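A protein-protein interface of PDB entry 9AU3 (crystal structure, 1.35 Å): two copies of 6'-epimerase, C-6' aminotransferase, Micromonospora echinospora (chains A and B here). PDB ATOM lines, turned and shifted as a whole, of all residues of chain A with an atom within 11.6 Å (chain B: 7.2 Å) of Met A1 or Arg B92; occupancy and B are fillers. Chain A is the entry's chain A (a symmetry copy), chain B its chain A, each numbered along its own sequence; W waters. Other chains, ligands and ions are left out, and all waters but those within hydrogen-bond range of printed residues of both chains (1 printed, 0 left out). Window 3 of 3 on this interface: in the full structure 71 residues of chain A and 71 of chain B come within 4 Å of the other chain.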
ATOM      1  N   MET A   1      19.299  26.214  -7.999  1.00  0.00           N
ATOM      2  CA  MET A   1      20.601  25.809  -8.511  1.00  0.00           C
ATOM      3  C   MET A   1      20.530  25.845 -10.028  1.00  0.00           C
ATOM      4  O   MET A   1      19.478  26.165 -10.585  1.00  0.00           O
ATOM      5  CB  MET A   1      20.938  24.408  -8.022  1.00  0.00           C
ATOM      6  CG  MET A   1      22.375  24.235  -7.592  1.00  0.00           C
ATOM      7  SD  MET A   1      22.597  22.635  -6.801  1.00  0.00           S
ATOM      8  CE  MET A   1      22.356  23.072  -5.081  1.00  0.00           C
ATOM      9  N   ILE A   2      21.625  25.522 -10.718  1.00  0.00           N
ATOM     10  CA  ILE A   2      21.580  25.645 -12.169  1.00  0.00           C
ATOM     11  C   ILE A   2      21.104  24.378 -12.863  1.00  0.00           C
ATOM     12  O   ILE A   2      20.804  24.439 -14.060  1.00  0.00           O
ATOM     13  CB  ILE A   2      22.911  25.971 -12.849  1.00  0.00           C
ATOM     14  CG1 ILE A   2      24.023  25.265 -12.131  1.00  0.00           C
ATOM     15  CG2 ILE A   2      23.168  27.473 -12.844  1.00  0.00           C
ATOM     16  CD1 ILE A   2      25.237  25.417 -12.856  1.00  0.00           C
ATOM     17  N   ILE A   3      21.082  23.236 -12.177  1.00  0.00           N
ATOM     18  CA  ILE A   3      20.537  22.020 -12.778  1.00  0.00           C
ATOM     19  C   ILE A   3      19.022  22.086 -12.698  1.00  0.00           C
ATOM     20  O   ILE A   3      18.442  22.068 -11.605  1.00  0.00           O
ATOM     21  CB  ILE A   3      21.060  20.747 -12.105  1.00  0.00           C
ATOM     22  CG1 ILE A   3      22.574  20.658 -12.207  1.00  0.00           C
ATOM     23  CG2 ILE A   3      20.422  19.521 -12.774  1.00  0.00           C
ATOM     24  CD1 ILE A   3      23.099  19.294 -11.887  1.00  0.00           C
ATOM     25  N   ALA A   4      18.381  22.140 -13.857  1.00  0.00           N
ATOM     26  CA  ALA A   4      16.947  22.366 -13.906  1.00  0.00           C
ATOM     27  C   ALA A   4      16.168  21.130 -13.499  1.00  0.00           C
ATOM     28  O   ALA A   4      15.075  21.258 -12.941  1.00  0.00           O
ATOM     29  CB  ALA A   4      16.543  22.812 -15.311  1.00  0.00           C
ATOM     30  N   ASN A   5      16.707  19.931 -13.750  1.00  0.00           N
ATOM     31  CA  ASN A   5      15.938  18.707 -13.535  1.00  0.00           C
ATOM     32  C   ASN A   5      16.483  17.824 -12.412  1.00  0.00           C
ATOM     33  O   ASN A   5      16.785  16.647 -12.619  1.00  0.00           O
ATOM     34  CB  ASN A   5      15.709  17.943 -14.855  1.00  0.00           C
ATOM     35  CG  ASN A   5      17.001  17.473 -15.537  1.00  0.00           C
ATOM     36  OD1 ASN A   5      18.103  17.984 -15.300  1.00  0.00           O
ATOM     37  ND2 ASN A   5      16.848  16.489 -16.411  1.00  0.00           N
ATOM     38  N   ALA A   6      16.582  18.370 -11.203  1.00  0.00           N
ATOM     39  CA  ALA A   6      17.004  17.591 -10.044  1.00  0.00           C
ATOM     40  C   ALA A   6      15.829  17.079  -9.208  1.00  0.00           C
ATOM     41  O   ALA A   6      16.029  16.675  -8.056  1.00  0.00           O
ATOM     42  CB  ALA A   6      17.983  18.393  -9.185  1.00  0.00           C
ATOM     43  N   ASP A   7      14.616  17.073  -9.764  1.00  0.00           N
ATOM     44  CA  ASP A   7      13.398  16.680  -9.065  1.00  0.00           C
ATOM     45  C   ASP A   7      12.903  15.329  -9.590  1.00  0.00           C
ATOM     46  O   ASP A   7      13.709  14.525 -10.091  1.00  0.00           O
ATOM     47  CB  ASP A   7      12.369  17.803  -9.187  1.00  0.00           C
ATOM     48  CG  ASP A   7      12.618  18.932  -8.211  1.00  0.00           C
ATOM     49  OD1 ASP A   7      12.977  18.648  -7.049  1.00  0.00           O
ATOM     50  OD2 ASP A   7      12.441  20.105  -8.602  1.00  0.00           O
ATOM     51  N   THR A  10      14.071  11.214  -8.765  1.00  0.00           N
ATOM     52  CA  THR A  10      15.465  11.177  -8.355  1.00  0.00           C
ATOM     53  C   THR A  10      15.579  10.438  -7.025  1.00  0.00           C
ATOM     54  O   THR A  10      14.823  10.726  -6.082  1.00  0.00           O
ATOM     55  CB  THR A  10      16.042  12.600  -8.269  1.00  0.00           C
ATOM     56  OG1 THR A  10      17.231  12.685  -9.065  1.00  0.00           O
ATOM     57  CG2 THR A  10      16.391  13.013  -6.852  1.00  0.00           C
ATOM     58  N   GLU A  13      16.373  10.821  -1.839  1.00  0.00           N
ATOM     59  CA  GLU A  13      15.896  12.089  -1.287  1.00  0.00           C
ATOM     60  C   GLU A  13      15.985  12.115   0.238  1.00  0.00           C
ATOM     61  O   GLU A  13      16.188  13.183   0.828  1.00  0.00           O
ATOM     62  CB  GLU A  13      14.450  12.339  -1.716  1.00  0.00           C
ATOM     63  CG  GLU A  13      14.257  13.139  -3.011  1.00  0.00           C
ATOM     64  CD  GLU A  13      15.165  14.352  -3.145  1.00  0.00           C
ATOM     65  OE1 GLU A  13      14.681  15.481  -2.917  1.00  0.00           O
ATOM     66  OE2 GLU A  13      16.345  14.185  -3.520  1.00  0.00           O
ATOM     67  N   ARG A  16      19.377  13.678   1.451  1.00  0.00           N
ATOM     68  CA  ARG A  16      19.842  14.960   0.933  1.00  0.00           C
ATOM     69  C   ARG A  16      20.561  15.796   1.987  1.00  0.00           C
ATOM     70  O   ARG A  16      21.227  16.775   1.626  1.00  0.00           O
ATOM     71  CB  ARG A  16      18.667  15.743   0.341  1.00  0.00           C
ATOM     72  CG  ARG A  16      18.253  15.305  -1.061  1.00  0.00           C
ATOM     73  CD  ARG A  16      19.354  15.499  -2.104  1.00  0.00           C
ATOM     74  NE  ARG A  16      18.966  14.929  -3.393  1.00  0.00           N
ATOM     75  CZ  ARG A  16      19.485  13.828  -3.922  1.00  0.00           C
ATOM     76  NH1 ARG A  16      20.478  13.179  -3.335  1.00  0.00           N
ATOM     77  NH2 ARG A  16      19.000  13.368  -5.071  1.00  0.00           N
ATOM     78  N   GLY A  17      20.440  15.446   3.265  1.00  0.00           N
ATOM     79  CA  GLY A  17      21.160  16.092   4.343  1.00  0.00           C
ATOM     80  C   GLY A  17      22.488  15.462   4.701  1.00  0.00           C
ATOM     81  O   GLY A  17      23.151  15.929   5.634  1.00  0.00           O
ATOM     82  N   VAL A  18      22.889  14.401   3.994  1.00  0.00           N
ATOM     83  CA  VAL A  18      24.196  13.771   4.141  1.00  0.00           C
ATOM     84  C   VAL A  18      24.814  13.623   2.750  1.00  0.00           C
ATOM     85  O   VAL A  18      24.182  13.914   1.735  1.00  0.00           O
ATOM     86  CB  VAL A  18      24.124  12.410   4.870  1.00  0.00           C
ATOM     87  CG1 VAL A  18      23.572  12.589   6.278  1.00  0.00           C
ATOM     88  CG2 VAL A  18      23.270  11.428   4.084  1.00  0.00           C
ATOM     89  N   LEU B  73      26.324  15.271  -6.222  1.00  0.00           N
ATOM     90  CA  LEU B  73      25.715  16.575  -6.471  1.00  0.00           C
ATOM     91  C   LEU B  73      26.746  17.603  -6.916  1.00  0.00           C
ATOM     92  O   LEU B  73      26.480  18.407  -7.818  1.00  0.00           O
ATOM     93  CB  LEU B  73      24.995  17.056  -5.211  1.00  0.00           C
ATOM     94  CG  LEU B  73      23.591  16.499  -4.956  1.00  0.00           C
ATOM     95  CD1 LEU B  73      23.655  15.109  -4.329  1.00  0.00           C
ATOM     96  CD2 LEU B  73      22.789  17.446  -4.078  1.00  0.00           C
ATOM     97  N   ASN B  77      26.445  19.468 -10.566  1.00  0.00           N
ATOM     98  CA  ASN B  77      26.345  20.920 -10.649  1.00  0.00           C
ATOM     99  C   ASN B  77      27.564  21.519 -11.329  1.00  0.00           C
ATOM    100  O   ASN B  77      27.446  22.508 -12.058  1.00  0.00           O
ATOM    101  CB  ASN B  77      26.142  21.536  -9.270  1.00  0.00           C
ATOM    102  CG  ASN B  77      25.649  22.962  -9.352  1.00  0.00           C
ATOM    103  OD1 ASN B  77      24.580  23.227  -9.901  1.00  0.00           O
ATOM    104  ND2 ASN B  77      26.433  23.890  -8.827  1.00  0.00           N
ATOM    105  N   ALA B  80      27.111  21.278 -15.032  1.00  0.00           N
ATOM    106  CA  ALA B  80      26.130  22.273 -15.453  1.00  0.00           C
ATOM    107  C   ALA B  80      26.759  23.659 -15.533  1.00  0.00           C
ATOM    108  O   ALA B  80      26.501  24.405 -16.485  1.00  0.00           O
ATOM    109  CB  ALA B  80      24.922  22.266 -14.510  1.00  0.00           C
ATOM    110  N   GLU B  81      27.594  24.010 -14.542  1.00  0.00           N
ATOM    111  CA  GLU B  81      28.296  25.294 -14.557  1.00  0.00           C
ATOM    112  C   GLU B  81      29.250  25.398 -15.743  1.00  0.00           C
ATOM    113  O   GLU B  81      29.393  26.473 -16.349  1.00  0.00           O
ATOM    114  CB  GLU B  81      29.089  25.479 -13.261  1.00  0.00           C
ATOM    115  CG  GLU B  81      28.285  25.927 -12.071  1.00  0.00           C
ATOM    116  CD  GLU B  81      28.993  25.730 -10.744  1.00  0.00           C
ATOM    117  OE1 GLU B  81      30.155  25.264 -10.732  1.00  0.00           O
ATOM    118  OE2 GLU B  81      28.379  26.060  -9.706  1.00  0.00           O
ATOM    119  N   ILE B  83      28.982  23.989 -18.674  1.00  0.00           N
ATOM    120  CA  ILE B  83      28.190  24.169 -19.885  1.00  0.00           C
ATOM    121  C   ILE B  83      27.577  25.566 -19.932  1.00  0.00           C
ATOM    122  O   ILE B  83      27.673  26.268 -20.941  1.00  0.00           O
ATOM    123  CB  ILE B  83      27.122  23.061 -19.958  1.00  0.00           C
ATOM    124  CG1 ILE B  83      27.797  21.706 -20.186  1.00  0.00           C
ATOM    125  CG2 ILE B  83      26.093  23.362 -21.043  1.00  0.00           C
ATOM    126  CD1 ILE B  83      26.863  20.518 -19.984  1.00  0.00           C
ATOM    127  N   ALA B  84      26.944  25.997 -18.843  1.00  0.00           N
ATOM    128  CA  ALA B  84      26.295  27.301 -18.850  1.00  0.00           C
ATOM    129  C   ALA B  84      27.309  28.422 -19.034  1.00  0.00           C
ATOM    130  O   ALA B  84      27.009  29.437 -19.681  1.00  0.00           O
ATOM    131  CB  ALA B  84      25.516  27.494 -17.547  1.00  0.00           C
ATOM    132  N   LEU B  87      28.088  29.765 -22.598  1.00  0.00           N
ATOM    133  CA  LEU B  87      27.013  30.369 -23.374  1.00  0.00           C
ATOM    134  C   LEU B  87      26.744  31.779 -22.878  1.00  0.00           C
ATOM    135  O   LEU B  87      26.767  32.027 -21.669  1.00  0.00           O
ATOM    136  CB  LEU B  87      25.717  29.566 -23.244  1.00  0.00           C
ATOM    137  CG  LEU B  87      25.763  28.223 -23.957  1.00  0.00           C
ATOM    138  CD1 LEU B  87      24.683  27.298 -23.407  1.00  0.00           C
ATOM    139  CD2 LEU B  87      25.592  28.415 -25.455  1.00  0.00           C
ATOM    140  N   GLY B  89      24.730  34.756 -21.513  1.00  0.00           N
ATOM    141  CA  GLY B  89      23.484  34.849 -20.786  1.00  0.00           C
ATOM    142  C   GLY B  89      23.482  33.965 -19.552  1.00  0.00           C
ATOM    143  O   GLY B  89      24.503  33.415 -19.133  1.00  0.00           O
ATOM    144  N   ASP B  90      22.303  33.846 -18.963  1.00  0.00           N
ATOM    145  CA  ASP B  90      22.109  33.134 -17.703  1.00  0.00           C
ATOM    146  C   ASP B  90      21.330  31.857 -18.018  1.00  0.00           C
ATOM    147  O   ASP B  90      20.106  31.891 -18.185  1.00  0.00           O
ATOM    148  CB  ASP B  90      21.357  34.048 -16.735  1.00  0.00           C
ATOM    149  CG  ASP B  90      21.250  33.475 -15.336  1.00  0.00           C
ATOM    150  OD1 ASP B  90      21.999  32.532 -15.010  1.00  0.00           O
ATOM    151  OD2 ASP B  90      20.443  34.014 -14.542  1.00  0.00           O
ATOM    152  N   GLN B  91      22.023  30.730 -18.099  1.00  0.00           N
ATOM    153  CA  GLN B  91      21.358  29.478 -18.439  1.00  0.00           C
ATOM    154  C   GLN B  91      21.221  28.556 -17.238  1.00  0.00           C
ATOM    155  O   GLN B  91      22.036  28.576 -16.311  1.00  0.00           O
ATOM    156  CB  GLN B  91      22.116  28.719 -19.538  1.00  0.00           C
ATOM    157  CG  GLN B  91      21.920  29.286 -20.931  1.00  0.00           C
ATOM    158  CD  GLN B  91      22.850  30.448 -21.189  1.00  0.00           C
ATOM    159  OE1 GLN B  91      23.879  30.594 -20.526  1.00  0.00           O
ATOM    160  NE2 GLN B  91      22.488  31.286 -22.142  1.00  0.00           N
ATOM    161  N   ARG B  92      20.183  27.732 -17.287  1.00  0.00           N
ATOM    162  CA  ARG B  92      20.077  26.522 -16.489  1.00  0.00           C
ATOM    163  C   ARG B  92      20.243  25.340 -17.433  1.00  0.00           C
ATOM    164  O   ARG B  92      20.145  25.490 -18.651  1.00  0.00           O
ATOM    165  CB  ARG B  92      18.715  26.446 -15.784  1.00  0.00           C
ATOM    166  CG  ARG B  92      18.384  27.650 -14.909  1.00  0.00           C
ATOM    167  CD  ARG B  92      19.379  27.818 -13.781  1.00  0.00           C
ATOM    168  NE  ARG B  92      19.045  28.950 -12.923  1.00  0.00           N
ATOM    169  CZ  ARG B  92      19.506  30.180 -13.100  1.00  0.00           C
ATOM    170  NH1 ARG B  92      20.373  30.463 -14.059  1.00  0.00           N
ATOM    171  NH2 ARG B  92      19.084  31.152 -12.298  1.00  0.00           N
ATOM    172  N   VAL B  93      20.535  24.167 -16.875  1.00  0.00           N
ATOM    173  CA  VAL B  93      20.879  22.995 -17.682  1.00  0.00           C
ATOM    174  C   VAL B  93      20.050  21.806 -17.218  1.00  0.00           C
ATOM    175  O   VAL B  93      20.032  21.487 -16.026  1.00  0.00           O
ATOM    176  CB  VAL B  93      22.386  22.669 -17.586  1.00  0.00           C
ATOM    177  CG1 VAL B  93      22.740  21.457 -18.455  1.00  0.00           C
ATOM    178  CG2 VAL B  93      23.231  23.881 -17.991  1.00  0.00           C
ATOM    179  N   ALA B  94      19.382  21.141 -18.157  1.00  0.00           N
ATOM    180  CA  ALA B  94      18.656  19.904 -17.879  1.00  0.00           C
ATOM    181  C   ALA B  94      19.342  18.768 -18.627  1.00  0.00           C
ATOM    182  O   ALA B  94      19.598  18.887 -19.827  1.00  0.00           O
ATOM    183  CB  ALA B  94      17.201  20.020 -18.338  1.00  0.00           C
ATOM    184  N   TYR B 223      19.635  25.711 -26.201  1.00  0.00           N
ATOM    185  CA  TYR B 223      20.665  25.003 -26.955  1.00  0.00           C
ATOM    186  C   TYR B 223      20.644  23.548 -26.522  1.00  0.00           C
ATOM    187  O   TYR B 223      20.439  23.251 -25.344  1.00  0.00           O
ATOM    188  CB  TYR B 223      22.048  25.561 -26.626  1.00  0.00           C
ATOM    189  CG  TYR B 223      22.207  27.056 -26.818  1.00  0.00           C
ATOM    190  CD1 TYR B 223      21.794  27.946 -25.843  1.00  0.00           C
ATOM    191  CD2 TYR B 223      22.815  27.571 -27.957  1.00  0.00           C
ATOM    192  CE1 TYR B 223      21.937  29.308 -26.005  1.00  0.00           C
ATOM    193  CE2 TYR B 223      22.981  28.936 -28.125  1.00  0.00           C
ATOM    194  CZ  TYR B 223      22.539  29.801 -27.149  1.00  0.00           C
ATOM    195  OH  TYR B 223      22.712  31.163 -27.307  1.00  0.00           O
ATOM    196  N   VAL B 238      19.797  20.082 -22.402  1.00  0.00           N
ATOM    197  CA  VAL B 238      19.205  21.346 -22.837  1.00  0.00           C
ATOM    198  C   VAL B 238      19.796  22.426 -21.941  1.00  0.00           C
ATOM    199  O   VAL B 238      19.721  22.325 -20.713  1.00  0.00           O
ATOM    200  CB  VAL B 238      17.672  21.330 -22.695  1.00  0.00           C
ATOM    201  CG1 VAL B 238      17.086  22.669 -23.155  1.00  0.00           C
ATOM    202  CG2 VAL B 238      17.047  20.175 -23.490  1.00  0.00           C
ATOM    203  N   ALA B 239      20.395  23.455 -22.535  1.00  0.00           N
ATOM    204  CA  ALA B 239      20.877  24.601 -21.777  1.00  0.00           C
ATOM    205  C   ALA B 239      20.125  25.816 -22.284  1.00  0.00           C
ATOM    206  O   ALA B 239      20.077  26.046 -23.492  1.00  0.00           O
ATOM    207  CB  ALA B 239      22.383  24.791 -21.954  1.00  0.00           C
ATOM    208  N   GLY B 240      19.530  26.586 -21.379  1.00  0.00           N
ATOM    209  CA  GLY B 240      18.734  27.696 -21.866  1.00  0.00           C
ATOM    210  C   GLY B 240      18.230  28.590 -20.756  1.00  0.00           C
ATOM    211  O   GLY B 240      18.504  28.387 -19.566  1.00  0.00           O
ATOM    212  N   ASP B 241      17.450  29.576 -21.174  1.00  0.00           N
ATOM    213  CA  ASP B 241      16.981  30.597 -20.254  1.00  0.00           C
ATOM    214  C   ASP B 241      16.047  29.975 -19.218  1.00  0.00           C
ATOM    215  O   ASP B 241      15.346  28.991 -19.481  1.00  0.00           O
ATOM    216  CB  ASP B 241      16.271  31.689 -21.052  1.00  0.00           C
ATOM    217  CG  ASP B 241      17.244  32.535 -21.880  1.00  0.00           C
ATOM    218  OD1 ASP B 241      18.474  32.303 -21.803  1.00  0.00           O
ATOM    219  OD2 ASP B 241      16.779  33.426 -22.619  1.00  0.00           O
ATOM    220  N   GLU B 242      16.064  30.553 -18.016  1.00  0.00           N
ATOM    221  CA  GLU B 242      15.349  29.981 -16.875  1.00  0.00           C
ATOM    222  C   GLU B 242      13.875  29.744 -17.180  1.00  0.00           C
ATOM    223  O   GLU B 242      13.297  28.746 -16.739  1.00  0.00           O
ATOM    224  CB  GLU B 242      15.482  30.934 -15.687  1.00  0.00           C
ATOM    225  CG  GLU B 242      14.749  30.499 -14.429  1.00  0.00           C
ATOM    226  CD  GLU B 242      15.222  31.249 -13.197  1.00  0.00           C
ATOM    227  OE1 GLU B 242      15.150  30.680 -12.089  1.00  0.00           O
ATOM    228  OE2 GLU B 242      15.658  32.411 -13.342  1.00  0.00           O
ATOM    229  N   ARG B 243      13.244  30.664 -17.912  1.00  0.00           N
ATOM    230  CA  ARG B 243      11.823  30.550 -18.226  1.00  0.00           C
ATOM    231  C   ARG B 243      11.508  29.251 -18.956  1.00  0.00           C
ATOM    232  O   ARG B 243      10.447  28.652 -18.744  1.00  0.00           O
ATOM    233  CB  ARG B 243      11.423  31.764 -19.070  1.00  0.00           C
ATOM    234  CG  ARG B 243      10.081  31.716 -19.773  1.00  0.00           C
ATOM    235  CD  ARG B 243       9.830  33.047 -20.496  1.00  0.00           C
ATOM    236  NE  ARG B 243       8.793  32.944 -21.515  1.00  0.00           N
ATOM    237  CZ  ARG B 243       8.868  33.491 -22.721  1.00  0.00           C
ATOM    238  NH1 ARG B 243       9.926  34.190 -23.101  1.00  0.00           N
ATOM    239  NH2 ARG B 243       7.860  33.317 -23.575  1.00  0.00           N
ATOM    240  N   LEU B 245      13.633  26.477 -18.930  1.00  0.00           N
ATOM    241  CA  LEU B 245      14.185  25.320 -18.245  1.00  0.00           C
ATOM    242  C   LEU B 245      13.369  24.922 -17.021  1.00  0.00           C
ATOM    243  O   LEU B 245      13.374  23.745 -16.638  1.00  0.00           O
ATOM    244  CB  LEU B 245      15.650  25.589 -17.883  1.00  0.00           C
ATOM    245  CG  LEU B 245      16.681  25.224 -18.964  1.00  0.00           C
ATOM    246  CD1 LEU B 245      16.948  23.728 -18.956  1.00  0.00           C
ATOM    247  CD2 LEU B 245      16.236  25.675 -20.367  1.00  0.00           C
ATOM    248  N   LYS B 246      12.664  25.869 -16.399  1.00  0.00           N
ATOM    249  CA  LYS B 246      11.813  25.528 -15.260  1.00  0.00           C
ATOM    250  C   LYS B 246      10.767  24.460 -15.583  1.00  0.00           C
ATOM    251  O   LYS B 246      10.564  23.562 -14.743  1.00  0.00           O
ATOM    252  CB  LYS B 246      11.225  26.813 -14.648  1.00  0.00           C
ATOM    253  CG  LYS B 246      10.133  26.611 -13.602  1.00  0.00           C
ATOM    254  CD  LYS B 246       8.807  27.249 -14.015  1.00  0.00           C
ATOM    255  CE  LYS B 246       7.962  26.317 -14.871  1.00  0.00           C
ATOM    256  NZ  LYS B 246       6.810  27.016 -15.516  1.00  0.00           N
HETATM  257  O   HOH W   1      13.757  23.519 -13.252  1.00  0.00           O
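N of Ala A4 is in hydrogen-bond range of O of Val B93 (2.8 Å). N of Val B93 lies within hydrogen-bond range of O of Ile A2, at 2.8 Å. The side-chain sulfur (SD) of Met A1 sits close to the side-chain amide oxygen (OD1) of Asn B77, 3.7 Å away.
The side-chain carboxylate (OD1) of Asp B90 is in salt-bridge range of the guanidinium group (NH1) of Arg B92 (2.8 Å). The backbone NH (N) of Arg B92 sits at hydrogen-bond distance from the backbone carbonyl oxygen (O) of Gly B240, at 2.9 Å. The backbone NH of Ala B94 is in hydrogen-bond range of the backbone carbonyl oxygen of Val B238. The backbone carbonyl oxygen of Leu B87 sits close to the side-chain amide oxygen of Gln B91, at 3.4 Å. The side-chain carboxylate (OE2) of Glu B81 is in hydrogen-bond range of the side-chain amide nitrogen (ND2) of Asn B77 (3.0 Å). The side-chain amide oxygen (OE1) of Gln B91 sits close to the backbone carbonyl oxygen (O) of Ala B84 (3.4 Å).
Among the printed residues, merely in contact across the chains: Ile A2 with Asn B77 (3.1 Å), Ile A2 with Glu B81 (3.2 Å), Asn A5 with Ala B94 (3.3 Å), Ile A2 with Arg B92 (3.3 Å), Ile A3 with Val B93 (3.3 Å), Ile A2 with Ala B80 (3.5 Å), Ala A4 with Leu B245 (3.6 Å), Met A1 with Arg B92 (3.6 Å), Ile A3 with Asn B77 (3.6 Å), Ile A3 with Ala B80 (3.7 Å), Ile A2 with Gln B91 (3.8 Å) and Arg A16 with Leu B73 (3.8 Å).
Printed residues of chain B within 4 Å of Met A1: Asn B77 (3.3 Å) and Arg B92 (3.6 Å). Arg B92 touches two residues of chain A. Ala B84 touches none of the printed residues of chain A. Of chain A, only Ile A2, Ile A3 and Ala A4 come within 4 Å of Val B93. No residue of chain A comes within 4 Å of Ala B239. No residue of chain A comes within 4 Å of Gly B240. No residue of chain A comes within 4 Å of Glu B242. Of the printed residues of chain A, Leu B245 touches Ala A4. Of the printed residues of chain B, Ile A3 touches Asn B77, Ala B80 and Val B93. Of the printed residues of chain A, Ala B80 touches Ile A2 and Ile A3. Printed residues of chain A within 4 Å of Asn B77: Met A1, Ile A2 and Ile A3. Printed residues of chain A within 4 Å of Glu B81: Ile A2 (3.2 Å). Of the printed residues of chain B, Ala A4 touches Val B93 (2.8 Å) and Leu B245 (3.6 Å). The nearest printed residue of chain B that does not touch Met A1 is Leu B73 (5.7 Å). The nearest printed residue of chain B that does not touch Asn A5 is Val B93 (4.1 Å).
Printed residues of chain B that touch a printed residue of chain A: Leu B73, Asn B77, Ala B80, Glu B81, Gln B91, Arg B92, Val B93, Ala B94 and Leu B245. Of the 12 printed residues of chain A, 6 touch a printed residue of chain B. Among the printed residues, 15 pairs touch across the chains.
No position is printed for both chains.
Water W1 lies within hydrogen-bond range of the backbone carbonyl oxygen (O) of Ala A4 (2.6 Å) and the backbone carbonyl oxygen (O) of Leu B245 (3.4 Å).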
